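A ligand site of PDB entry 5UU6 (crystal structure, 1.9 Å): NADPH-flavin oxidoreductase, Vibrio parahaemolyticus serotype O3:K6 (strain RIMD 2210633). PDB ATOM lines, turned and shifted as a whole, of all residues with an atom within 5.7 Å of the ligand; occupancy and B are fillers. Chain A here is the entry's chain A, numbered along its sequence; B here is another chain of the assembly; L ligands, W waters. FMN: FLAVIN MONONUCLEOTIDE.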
ATOM      1  N   HIS A  14      22.945  36.450 -32.940  1.00  0.00           N
ATOM      2  CA  HIS A  14      22.474  35.103 -32.618  1.00  0.00           C
ATOM      3  C   HIS A  14      21.148  34.778 -33.301  1.00  0.00           C
ATOM      4  O   HIS A  14      20.199  35.573 -33.244  1.00  0.00           O
ATOM      5  CB  HIS A  14      22.280  34.960 -31.120  1.00  0.00           C
ATOM      6  CG  HIS A  14      21.419  33.787 -30.777  1.00  0.00           C
ATOM      7  ND1 HIS A  14      21.848  32.489 -30.950  1.00  0.00           N
ATOM      8  CD2 HIS A  14      20.140  33.712 -30.349  1.00  0.00           C
ATOM      9  CE1 HIS A  14      20.883  31.652 -30.594  1.00  0.00           C
ATOM     10  NE2 HIS A  14      19.835  32.371 -30.230  1.00  0.00           N
ATOM     11  N   ARG A  15      21.073  33.587 -33.902  1.00  0.00           N
ATOM     12  CA  ARG A  15      19.853  32.955 -34.372  1.00  0.00           C
ATOM     13  C   ARG A  15      19.898  31.498 -33.982  1.00  0.00           C
ATOM     14  O   ARG A  15      20.950  30.859 -34.133  1.00  0.00           O
ATOM     15  CB  ARG A  15      19.695  33.016 -35.909  1.00  0.00           C
ATOM     16  CG  ARG A  15      19.439  34.381 -36.484  1.00  0.00           C
ATOM     17  CD  ARG A  15      20.744  34.993 -36.958  1.00  0.00           C
ATOM     18  NE  ARG A  15      21.357  34.216 -38.038  1.00  0.00           N
ATOM     19  CZ  ARG A  15      22.570  33.668 -37.952  1.00  0.00           C
ATOM     20  NH1 ARG A  15      23.279  33.787 -36.834  1.00  0.00           N
ATOM     21  NH2 ARG A  15      23.063  32.988 -38.985  1.00  0.00           N
ATOM     22  N   SER A  16      18.758  30.961 -33.547  1.00  0.00           N
ATOM     23  CA  SER A  16      18.617  29.522 -33.463  1.00  0.00           C
ATOM     24  C   SER A  16      18.726  28.900 -34.850  1.00  0.00           C
ATOM     25  O   SER A  16      18.015  29.309 -35.780  1.00  0.00           O
ATOM     26  CB  SER A  16      17.288  29.157 -32.823  1.00  0.00           C
ATOM     27  OG  SER A  16      17.333  29.484 -31.449  1.00  0.00           O
ATOM     28  N   ARG A  18      18.328  25.418 -36.960  1.00  0.00           N
ATOM     29  CA  ARG A  18      17.650  24.133 -36.858  1.00  0.00           C
ATOM     30  C   ARG A  18      17.828  23.300 -38.115  1.00  0.00           C
ATOM     31  O   ARG A  18      17.065  22.380 -38.346  1.00  0.00           O
ATOM     32  CB  ARG A  18      16.164  24.303 -36.570  1.00  0.00           C
ATOM     33  CG  ARG A  18      15.910  25.121 -35.275  1.00  0.00           C
ATOM     34  CD  ARG A  18      14.411  25.247 -35.008  1.00  0.00           C
ATOM     35  NE  ARG A  18      14.144  25.950 -33.763  1.00  0.00           N
ATOM     36  CZ  ARG A  18      14.084  27.274 -33.630  1.00  0.00           C
ATOM     37  NH1 ARG A  18      14.252  28.059 -34.690  1.00  0.00           N
ATOM     38  NH2 ARG A  18      13.806  27.812 -32.443  1.00  0.00           N
ATOM     39  N   ALA A  67      12.282  14.300 -27.750  1.00  0.00           N
ATOM     40  CA  ALA A  67      12.262  15.756 -27.787  1.00  0.00           C
ATOM     41  C   ALA A  67      11.040  16.291 -28.502  1.00  0.00           C
ATOM     42  O   ALA A  67      10.843  17.517 -28.557  1.00  0.00           O
ATOM     43  CB  ALA A  67      13.525  16.292 -28.494  1.00  0.00           C
ATOM     44  N   GLN A  70      11.917  16.180 -33.107  1.00  0.00           N
ATOM     45  CA  GLN A  70      12.683  17.295 -33.646  1.00  0.00           C
ATOM     46  C   GLN A  70      13.841  16.687 -34.408  1.00  0.00           C
ATOM     47  O   GLN A  70      14.815  16.215 -33.798  1.00  0.00           O
ATOM     48  CB  GLN A  70      13.148  18.212 -32.507  1.00  0.00           C
ATOM     49  CG  GLN A  70      11.965  18.743 -31.687  1.00  0.00           C
ATOM     50  CD  GLN A  70      12.327  19.917 -30.770  1.00  0.00           C
ATOM     51  OE1 GLN A  70      12.904  20.910 -31.218  1.00  0.00           O
ATOM     52  NE2 GLN A  70      11.983  19.807 -29.486  1.00  0.00           N
ATOM     53  N   TYR A  72      16.340  17.715 -36.048  1.00  0.00           N
ATOM     54  CA  TYR A  72      17.686  18.267 -35.986  1.00  0.00           C
ATOM     55  C   TYR A  72      18.439  17.731 -34.783  1.00  0.00           C
ATOM     56  O   TYR A  72      19.677  17.792 -34.757  1.00  0.00           O
ATOM     57  CB  TYR A  72      17.650  19.812 -35.980  1.00  0.00           C
ATOM     58  CG  TYR A  72      16.426  20.439 -35.356  1.00  0.00           C
ATOM     59  CD1 TYR A  72      15.250  20.606 -36.104  1.00  0.00           C
ATOM     60  CD2 TYR A  72      16.443  20.893 -34.037  1.00  0.00           C
ATOM     61  CE1 TYR A  72      14.116  21.140 -35.541  1.00  0.00           C
ATOM     62  CE2 TYR A  72      15.307  21.478 -33.467  1.00  0.00           C
ATOM     63  CZ  TYR A  72      14.159  21.610 -34.237  1.00  0.00           C
ATOM     64  OH  TYR A  72      13.037  22.157 -33.674  1.00  0.00           O
ATOM     65  N   VAL A 130      20.972  25.331 -31.390  1.00  0.00           N
ATOM     66  CA  VAL A 130      19.682  25.618 -30.761  1.00  0.00           C
ATOM     67  C   VAL A 130      19.598  24.806 -29.477  1.00  0.00           C
ATOM     68  O   VAL A 130      20.073  23.667 -29.409  1.00  0.00           O
ATOM     69  CB  VAL A 130      18.511  25.340 -31.760  1.00  0.00           C
ATOM     70  CG1 VAL A 130      18.467  23.868 -32.293  1.00  0.00           C
ATOM     71  CG2 VAL A 130      17.169  25.729 -31.170  1.00  0.00           C
ATOM     72  N   TYR A 131      19.039  25.421 -28.436  1.00  0.00           N
ATOM     73  CA  TYR A 131      18.669  24.695 -27.221  1.00  0.00           C
ATOM     74  C   TYR A 131      17.497  23.753 -27.503  1.00  0.00           C
ATOM     75  O   TYR A 131      16.603  24.090 -28.272  1.00  0.00           O
ATOM     76  CB  TYR A 131      18.253  25.675 -26.110  1.00  0.00           C
ATOM     77  CG  TYR A 131      19.372  26.531 -25.537  1.00  0.00           C
ATOM     78  CD1 TYR A 131      19.741  27.738 -26.133  1.00  0.00           C
ATOM     79  CD2 TYR A 131      20.058  26.134 -24.380  1.00  0.00           C
ATOM     80  CE1 TYR A 131      20.782  28.507 -25.621  1.00  0.00           C
ATOM     81  CE2 TYR A 131      21.069  26.917 -23.839  1.00  0.00           C
ATOM     82  CZ  TYR A 131      21.440  28.074 -24.471  1.00  0.00           C
ATOM     83  OH  TYR A 131      22.460  28.808 -23.930  1.00  0.00           O
ATOM     84  N   ILE A 132      17.480  22.596 -26.847  1.00  0.00           N
ATOM     85  CA  ILE A 132      16.375  21.635 -26.962  1.00  0.00           C
ATOM     86  C   ILE A 132      15.814  21.367 -25.567  1.00  0.00           C
ATOM     87  O   ILE A 132      16.202  20.426 -24.865  1.00  0.00           O
ATOM     88  CB  ILE A 132      16.818  20.337 -27.630  1.00  0.00           C
ATOM     89  CG1 ILE A 132      17.541  20.597 -28.973  1.00  0.00           C
ATOM     90  CG2 ILE A 132      15.611  19.376 -27.784  1.00  0.00           C
ATOM     91  CD1 ILE A 132      16.693  21.287 -30.137  1.00  0.00           C
ATOM     92  N   GLY A 133      14.882  22.200 -25.142  1.00  0.00           N
ATOM     93  CA  GLY A 133      14.175  21.914 -23.899  1.00  0.00           C
ATOM     94  C   GLY A 133      13.116  20.862 -24.087  1.00  0.00           C
ATOM     95  O   GLY A 133      12.529  20.379 -23.117  1.00  0.00           O
ATOM     96  N   GLY A 134      12.899  20.477 -25.328  1.00  0.00           N
ATOM     97  CA  GLY A 134      11.846  19.510 -25.657  1.00  0.00           C
ATOM     98  C   GLY A 134      12.095  18.143 -25.060  1.00  0.00           C
ATOM     99  O   GLY A 134      11.133  17.371 -24.881  1.00  0.00           O
ATOM    100  N   LEU A 135      13.360  17.837 -24.727  1.00  0.00           N
ATOM    101  CA  LEU A 135      13.698  16.620 -23.990  1.00  0.00           C
ATOM    102  C   LEU A 135      12.861  16.440 -22.735  1.00  0.00           C
ATOM    103  O   LEU A 135      12.529  15.304 -22.366  1.00  0.00           O
ATOM    104  CB  LEU A 135      15.169  16.652 -23.604  1.00  0.00           C
ATOM    105  CG  LEU A 135      16.169  16.578 -24.746  1.00  0.00           C
ATOM    106  CD1 LEU A 135      17.534  16.421 -24.111  1.00  0.00           C
ATOM    107  CD2 LEU A 135      15.816  15.395 -25.643  1.00  0.00           C
ATOM    108  N   ARG A 136      12.532  17.537 -22.058  1.00  0.00           N
ATOM    109  CA  ARG A 136      11.675  17.486 -20.864  1.00  0.00           C
ATOM    110  C   ARG A 136      10.262  17.015 -21.136  1.00  0.00           C
ATOM    111  O   ARG A 136       9.577  16.687 -20.183  1.00  0.00           O
ATOM    112  CB  ARG A 136      11.634  18.866 -20.180  1.00  0.00           C
ATOM    113  CG  ARG A 136      13.041  19.385 -19.795  1.00  0.00           C
ATOM    114  CD  ARG A 136      12.953  20.361 -18.631  1.00  0.00           C
ATOM    115  NE  ARG A 136      12.175  21.524 -19.001  1.00  0.00           N
ATOM    116  CZ  ARG A 136      12.686  22.598 -19.631  1.00  0.00           C
ATOM    117  NH1 ARG A 136      13.972  22.653 -19.960  1.00  0.00           N
ATOM    118  NH2 ARG A 136      11.890  23.612 -19.923  1.00  0.00           N
ATOM    119  N   PHE A 156      18.113  20.306 -20.404  1.00  0.00           N
ATOM    120  CA  PHE A 156      17.852  20.599 -21.823  1.00  0.00           C
ATOM    121  C   PHE A 156      19.021  20.066 -22.642  1.00  0.00           C
ATOM    122  O   PHE A 156      20.111  19.792 -22.119  1.00  0.00           O
ATOM    123  CB  PHE A 156      17.691  22.112 -22.075  1.00  0.00           C
ATOM    124  CG  PHE A 156      18.862  22.917 -21.574  1.00  0.00           C
ATOM    125  CD1 PHE A 156      19.978  23.097 -22.378  1.00  0.00           C
ATOM    126  CD2 PHE A 156      18.879  23.402 -20.262  1.00  0.00           C
ATOM    127  CE1 PHE A 156      21.113  23.794 -21.891  1.00  0.00           C
ATOM    128  CE2 PHE A 156      20.021  24.100 -19.768  1.00  0.00           C
ATOM    129  CZ  PHE A 156      21.128  24.289 -20.593  1.00  0.00           C
ATOM    130  N   GLU A 168      16.491  35.378 -40.113  1.00  0.00           N
ATOM    131  CA  GLU A 168      16.682  36.727 -39.634  1.00  0.00           C
ATOM    132  C   GLU A 168      16.678  36.715 -38.127  1.00  0.00           C
ATOM    133  O   GLU A 168      16.089  35.839 -37.501  1.00  0.00           O
ATOM    134  CB  GLU A 168      15.581  37.642 -40.173  1.00  0.00           C
ATOM    135  N   LYS A 170      15.538  37.451 -34.612  1.00  0.00           N
ATOM    136  CA  LYS A 170      14.175  37.613 -34.144  1.00  0.00           C
ATOM    137  C   LYS A 170      14.124  38.648 -33.031  1.00  0.00           C
ATOM    138  O   LYS A 170      14.949  38.600 -32.102  1.00  0.00           O
ATOM    139  CB  LYS A 170      13.649  36.272 -33.679  1.00  0.00           C
ATOM    140  CG  LYS A 170      12.335  36.298 -32.987  1.00  0.00           C
ATOM    141  CD  LYS A 170      11.929  34.901 -32.519  1.00  0.00           C
ATOM    142  CE  LYS A 170      12.379  33.782 -33.447  1.00  0.00           C
ATOM    143  NZ  LYS A 170      11.668  32.517 -33.082  1.00  0.00           N
ATOM    144  N   ARG A 172      13.034  40.908 -29.682  1.00  0.00           N
ATOM    145  CA  ARG A 172      12.578  40.651 -28.326  1.00  0.00           C
ATOM    146  C   ARG A 172      11.777  41.837 -27.832  1.00  0.00           C
ATOM    147  O   ARG A 172      11.797  42.912 -28.432  1.00  0.00           O
ATOM    148  CB  ARG A 172      13.780  40.416 -27.403  1.00  0.00           C
ATOM    149  CG  ARG A 172      14.112  38.980 -27.170  1.00  0.00           C
ATOM    150  CD  ARG A 172      14.756  38.415 -28.383  1.00  0.00           C
ATOM    151  NE  ARG A 172      15.325  37.099 -28.100  1.00  0.00           N
ATOM    152  CZ  ARG A 172      15.831  36.298 -29.035  1.00  0.00           C
ATOM    153  NH1 ARG A 172      15.772  36.651 -30.311  1.00  0.00           N
ATOM    154  NH2 ARG A 172      16.356  35.135 -28.707  1.00  0.00           N
ATOM    155  N   ALA B  39      19.367  39.654 -26.478  1.00  0.00           N
ATOM    156  CA  ALA B  39      19.589  38.735 -27.603  1.00  0.00           C
ATOM    157  C   ALA B  39      19.767  37.265 -27.189  1.00  0.00           C
ATOM    158  O   ALA B  39      20.045  36.426 -28.053  1.00  0.00           O
ATOM    159  CB  ALA B  39      20.806  39.201 -28.394  1.00  0.00           C
ATOM    160  N   ALA B  40      19.637  36.924 -25.907  1.00  0.00           N
ATOM    161  CA  ALA B  40      19.698  35.531 -25.475  1.00  0.00           C
ATOM    162  C   ALA B  40      18.537  34.708 -26.040  1.00  0.00           C
ATOM    163  O   ALA B  40      17.416  35.215 -26.199  1.00  0.00           O
ATOM    164  CB  ALA B  40      19.655  35.470 -23.946  1.00  0.00           C
ATOM    165  N   SER B  41      18.799  33.429 -26.334  1.00  0.00           N
ATOM    166  CA  SER B  41      17.712  32.463 -26.598  1.00  0.00           C
ATOM    167  C   SER B  41      16.725  32.447 -25.421  1.00  0.00           C
ATOM    168  O   SER B  41      17.099  32.722 -24.278  1.00  0.00           O
ATOM    169  CB  SER B  41      18.241  31.033 -26.774  1.00  0.00           C
ATOM    170  OG  SER B  41      19.184  30.895 -27.831  1.00  0.00           O
ATOM    171  N   SER B  42      15.502  31.995 -25.706  1.00  0.00           N
ATOM    172  CA  SER B  42      14.377  32.016 -24.758  1.00  0.00           C
ATOM    173  C   SER B  42      13.463  30.810 -25.022  1.00  0.00           C
ATOM    174  O   SER B  42      12.924  30.674 -26.124  1.00  0.00           O
ATOM    175  CB  SER B  42      13.606  33.350 -24.936  1.00  0.00           C
ATOM    176  OG  SER B  42      12.381  33.364 -24.233  1.00  0.00           O
ATOM    177  N   SER B  43      13.261  29.937 -24.011  1.00  0.00           N
ATOM    178  CA  SER B  43      12.324  28.817 -24.168  1.00  0.00           C
ATOM    179  C   SER B  43      10.964  29.280 -24.695  1.00  0.00           C
ATOM    180  O   SER B  43      10.329  30.162 -24.124  1.00  0.00           O
ATOM    181  CB  SER B  43      12.112  28.111 -22.816  1.00  0.00           C
ATOM    182  OG  SER B  43      13.356  27.847 -22.177  1.00  0.00           O
ATOM    183  N   SER B  44      10.529  28.675 -25.797  1.00  0.00           N
ATOM    184  CA  SER B  44       9.212  28.954 -26.391  1.00  0.00           C
ATOM    185  C   SER B  44       8.979  30.431 -26.634  1.00  0.00           C
ATOM    186  O   SER B  44       7.830  30.870 -26.765  1.00  0.00           O
ATOM    187  CB  SER B  44       8.082  28.392 -25.526  1.00  0.00           C
ATOM    188  OG  SER B  44       8.217  26.988 -25.372  1.00  0.00           O
ATOM    189  N   MET B  45      10.051  31.214 -26.710  1.00  0.00           N
ATOM    190  CA  MET B  45       9.961  32.687 -26.781  1.00  0.00           C
ATOM    191  C   MET B  45       9.079  33.266 -25.687  1.00  0.00           C
ATOM    192  O   MET B  45       8.408  34.285 -25.892  1.00  0.00           O
ATOM    193  CB  MET B  45       9.447  33.163 -28.148  1.00  0.00           C
ATOM    194  CG  MET B  45      10.563  33.254 -29.122  1.00  0.00           C
ATOM    195  SD  MET B  45      11.463  34.872 -28.663  1.00  0.00           S
ATOM    196  CE  MET B  45      10.325  36.041 -29.694  1.00  0.00           C
ATOM    197  N   VAL B 109      16.839  28.760 -15.918  1.00  0.00           N
ATOM    198  CA  VAL B 109      17.781  28.521 -17.024  1.00  0.00           C
ATOM    199  C   VAL B 109      17.918  29.766 -17.882  1.00  0.00           C
ATOM    200  O   VAL B 109      19.041  30.227 -18.196  1.00  0.00           O
ATOM    201  CB  VAL B 109      17.362  27.313 -17.877  1.00  0.00           C
ATOM    202  CG1 VAL B 109      18.128  27.297 -19.224  1.00  0.00           C
ATOM    203  CG2 VAL B 109      17.626  26.030 -17.167  1.00  0.00           C
ATOM    204  N   ASP B 110      16.779  30.364 -18.259  1.00  0.00           N
ATOM    205  CA  ASP B 110      16.819  31.519 -19.142  1.00  0.00           C
ATOM    206  C   ASP B 110      17.495  32.710 -18.482  1.00  0.00           C
ATOM    207  O   ASP B 110      18.207  33.469 -19.170  1.00  0.00           O
ATOM    208  CB  ASP B 110      15.400  31.887 -19.605  1.00  0.00           C
ATOM    209  CG  ASP B 110      14.801  30.828 -20.621  1.00  0.00           C
ATOM    210  OD1 ASP B 110      15.327  29.671 -20.675  1.00  0.00           O
ATOM    211  OD2 ASP B 110      13.823  31.158 -21.359  1.00  0.00           O
ATOM    212  N   ILE B 113      21.203  32.183 -18.898  1.00  0.00           N
ATOM    213  CA  ILE B 113      21.601  32.438 -20.281  1.00  0.00           C
ATOM    214  C   ILE B 113      21.727  33.928 -20.534  1.00  0.00           C
ATOM    215  O   ILE B 113      22.691  34.390 -21.120  1.00  0.00           O
ATOM    216  CB  ILE B 113      20.593  31.795 -21.245  1.00  0.00           C
ATOM    217  CG1 ILE B 113      20.646  30.262 -21.125  1.00  0.00           C
ATOM    218  CG2 ILE B 113      20.847  32.246 -22.721  1.00  0.00           C
ATOM    219  CD1 ILE B 113      19.572  29.604 -21.988  1.00  0.00           C
HETATM  220  N1  FMN L   1      13.888  25.526 -29.959  1.00  0.00           N
HETATM  221  C2  FMN L   1      13.342  24.412 -30.567  1.00  0.00           C
HETATM  222  O2  FMN L   1      13.119  24.445 -31.784  1.00  0.00           O
HETATM  223  N3  FMN L   1      13.064  23.272 -29.832  1.00  0.00           N
HETATM  224  C4  FMN L   1      13.330  23.225 -28.468  1.00  0.00           C
HETATM  225  O4  FMN L   1      13.086  22.195 -27.803  1.00  0.00           O
HETATM  226  C4A FMN L   1      13.864  24.368 -27.838  1.00  0.00           C
HETATM  227  N5  FMN L   1      14.135  24.404 -26.481  1.00  0.00           N
HETATM  228  C5A FMN L   1      14.715  25.495 -25.875  1.00  0.00           C
HETATM  229  C6  FMN L   1      15.021  25.467 -24.512  1.00  0.00           C
HETATM  230  C7  FMN L   1      15.599  26.598 -23.927  1.00  0.00           C
HETATM  231  C7M FMN L   1      15.950  26.609 -22.459  1.00  0.00           C
HETATM  232  C8  FMN L   1      15.871  27.727 -24.669  1.00  0.00           C
HETATM  233  C8M FMN L   1      16.478  28.945 -23.999  1.00  0.00           C
HETATM  234  C9  FMN L   1      15.563  27.765 -26.046  1.00  0.00           C
HETATM  235  C9A FMN L   1      14.983  26.643 -26.631  1.00  0.00           C
HETATM  236  N10 FMN L   1      14.692  26.634 -28.002  1.00  0.00           N
HETATM  237  C10 FMN L   1      14.155  25.511 -28.602  1.00  0.00           C
HETATM  238  C1' FMN L   1      14.987  27.810 -28.879  1.00  0.00           C
HETATM  239  C2' FMN L   1      13.860  28.842 -28.758  1.00  0.00           C
HETATM  240  O2' FMN L   1      12.739  28.397 -29.483  1.00  0.00           O
HETATM  241  C3' FMN L   1      14.425  30.161 -29.288  1.00  0.00           C
HETATM  242  O3' FMN L   1      15.437  30.663 -28.431  1.00  0.00           O
HETATM  243  C4' FMN L   1      13.418  31.245 -29.637  1.00  0.00           C
HETATM  244  O4' FMN L   1      12.175  30.739 -30.006  1.00  0.00           O
HETATM  245  C5' FMN L   1      13.893  31.587 -31.000  1.00  0.00           C
HETATM  246  O5' FMN L   1      14.597  32.763 -30.963  1.00  0.00           O
HETATM  247  P   FMN L   1      16.121  32.798 -31.463  1.00  0.00           P
HETATM  248  O1P FMN L   1      16.301  32.489 -32.943  1.00  0.00           O
HETATM  249  O2P FMN L   1      16.486  34.239 -31.286  1.00  0.00           O
HETATM  250  O3P FMN L   1      17.001  31.874 -30.620  1.00  0.00           O
HETATM  251  O   HOH W   1      14.041  30.821 -33.813  1.00  0.00           O
HETATM  252  O   HOH W   2      16.166  33.388 -35.634  1.00  0.00           O
HETATM  253  O   HOH W   3      13.177  25.005 -21.671  1.00  0.00           O
HETATM  254  O   HOH W   4      11.151  26.777 -28.280  1.00  0.00           O
HETATM  255  O   HOH W   5       9.727  21.748 -27.003  1.00  0.00           O
HETATM  256  O   HOH W   6      17.526  35.583 -33.189  1.00  0.00           O
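The side-chain amide oxygen (OE1) of Gln 70 sits at hydrogen-bond distance from the side-chain hydroxyl (OH) of Tyr 72, 2.8 Å away.
The guanidinium group (NH1) of Arg 172 is in hydrogen-bond range of the backbone carbonyl oxygen (O) of Lys 170, 2.8 Å away.
The backbone carbonyl oxygen of Ala 67 is in hydrogen-bond range of the side-chain amide nitrogen of Gln 70, at 2.7 Å.
A ring nitrogen (NE2) of His 14 lies within hydrogen-bond range of the side-chain hydroxyl (OG) of Ser 41 of chain B, at 2.9 Å.
The backbone NH of Ser 43 of chain B lies within hydrogen-bond range of the side-chain carboxylate of Asp 110 of chain B, at 3.0 Å.
The guanidinium group (NH2) of Arg 172 sits at hydrogen-bond distance from the backbone carbonyl oxygen (O) of Ala 40 of chain B, 2.7 Å away.
The backbone carbonyl oxygen (O) of Tyr 131 lies close to a nitrogen (N5) of the ligand, 3.1 Å away.
Merely in contact with the ligand: Ser 43 of chain B (2.9 Å), Met 45 of chain B (3.1 Å), Lys 170 (3.2 Å), Ser 41 of chain B (3.3 Å), Ile 132 (3.4 Å), Val 130 (3.5 Å), Asp 110 of chain B (3.6 Å), Ile 113 of chain B (3.7 Å), Arg 15 (3.9 Å) and Val 109 of chain B (3.96 Å).
Of the 28 residues printed, 20 come within 4 Å of the ligand.
The nearest printed residue that does not touch the ligand is Ser 44 of chain B (4.3 Å).
The side-chain hydroxyl (OG) of Ser 16 is in hydrogen-bond range of an oxygen (O3P) of the ligand (2.6 Å).
An oxygen (O4) of the ligand sits at hydrogen-bond distance from the backbone NH of Gly 134, at 3.0 Å.
An oxygen (O2) of the ligand lies within hydrogen-bond range of the side-chain hydroxyl (OH) of Tyr 72 (3.0 Å).
A nitrogen (N3) of the ligand sits at hydrogen-bond distance from the side-chain amide oxygen (OE1) of Gln 70, 2.7 Å away.
NE of Arg 18 is in hydrogen-bond range of O2 of the ligand, at 2.7 Å.
The backbone NH (N) of Gly 133 sits at hydrogen-bond distance from a nitrogen (N5) of the ligand, 2.7 Å away.
O3P of the ligand lies within hydrogen-bond range of NE2 of His 14 (2.9 Å).
An oxygen (O3') of the ligand sits close to the backbone carbonyl oxygen (O) of Ser 42 of chain B.
O1P of the ligand sits at hydrogen-bond distance from N of Ser 16, at 3.0 Å.
O2P of the ligand is in salt-bridge range of NH1 of Arg 172 (2.7 Å).
The backbone NH (N) of Ser 42 of chain B sits at hydrogen-bond distance from an oxygen (O3') of the ligand (3.0 Å).
Water W6 lies within hydrogen-bond range of an oxygen (O2P) of the ligand (2.6 Å), the backbone carbonyl oxygen (O) of His 14 (2.7 Å) and the backbone NH (N) of Lys 170 (3.1 Å).
Water W4 lies within hydrogen-bond range of O2' of the ligand and N of Ser 44 of chain B.
Water W2 bridges O1P of the ligand (2.8 Å) and O of Glu 168 (3.1 Å).
Water W1 lies within hydrogen-bond range of NH1 of Arg 18, O1P of the ligand and NZ of Lys 170.
Water W3 lies within hydrogen-bond range of the guanidinium group (NH2) of Arg 136 (2.6 Å) and the side-chain hydroxyl (OG) of Ser 43 of chain B (2.9 Å).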
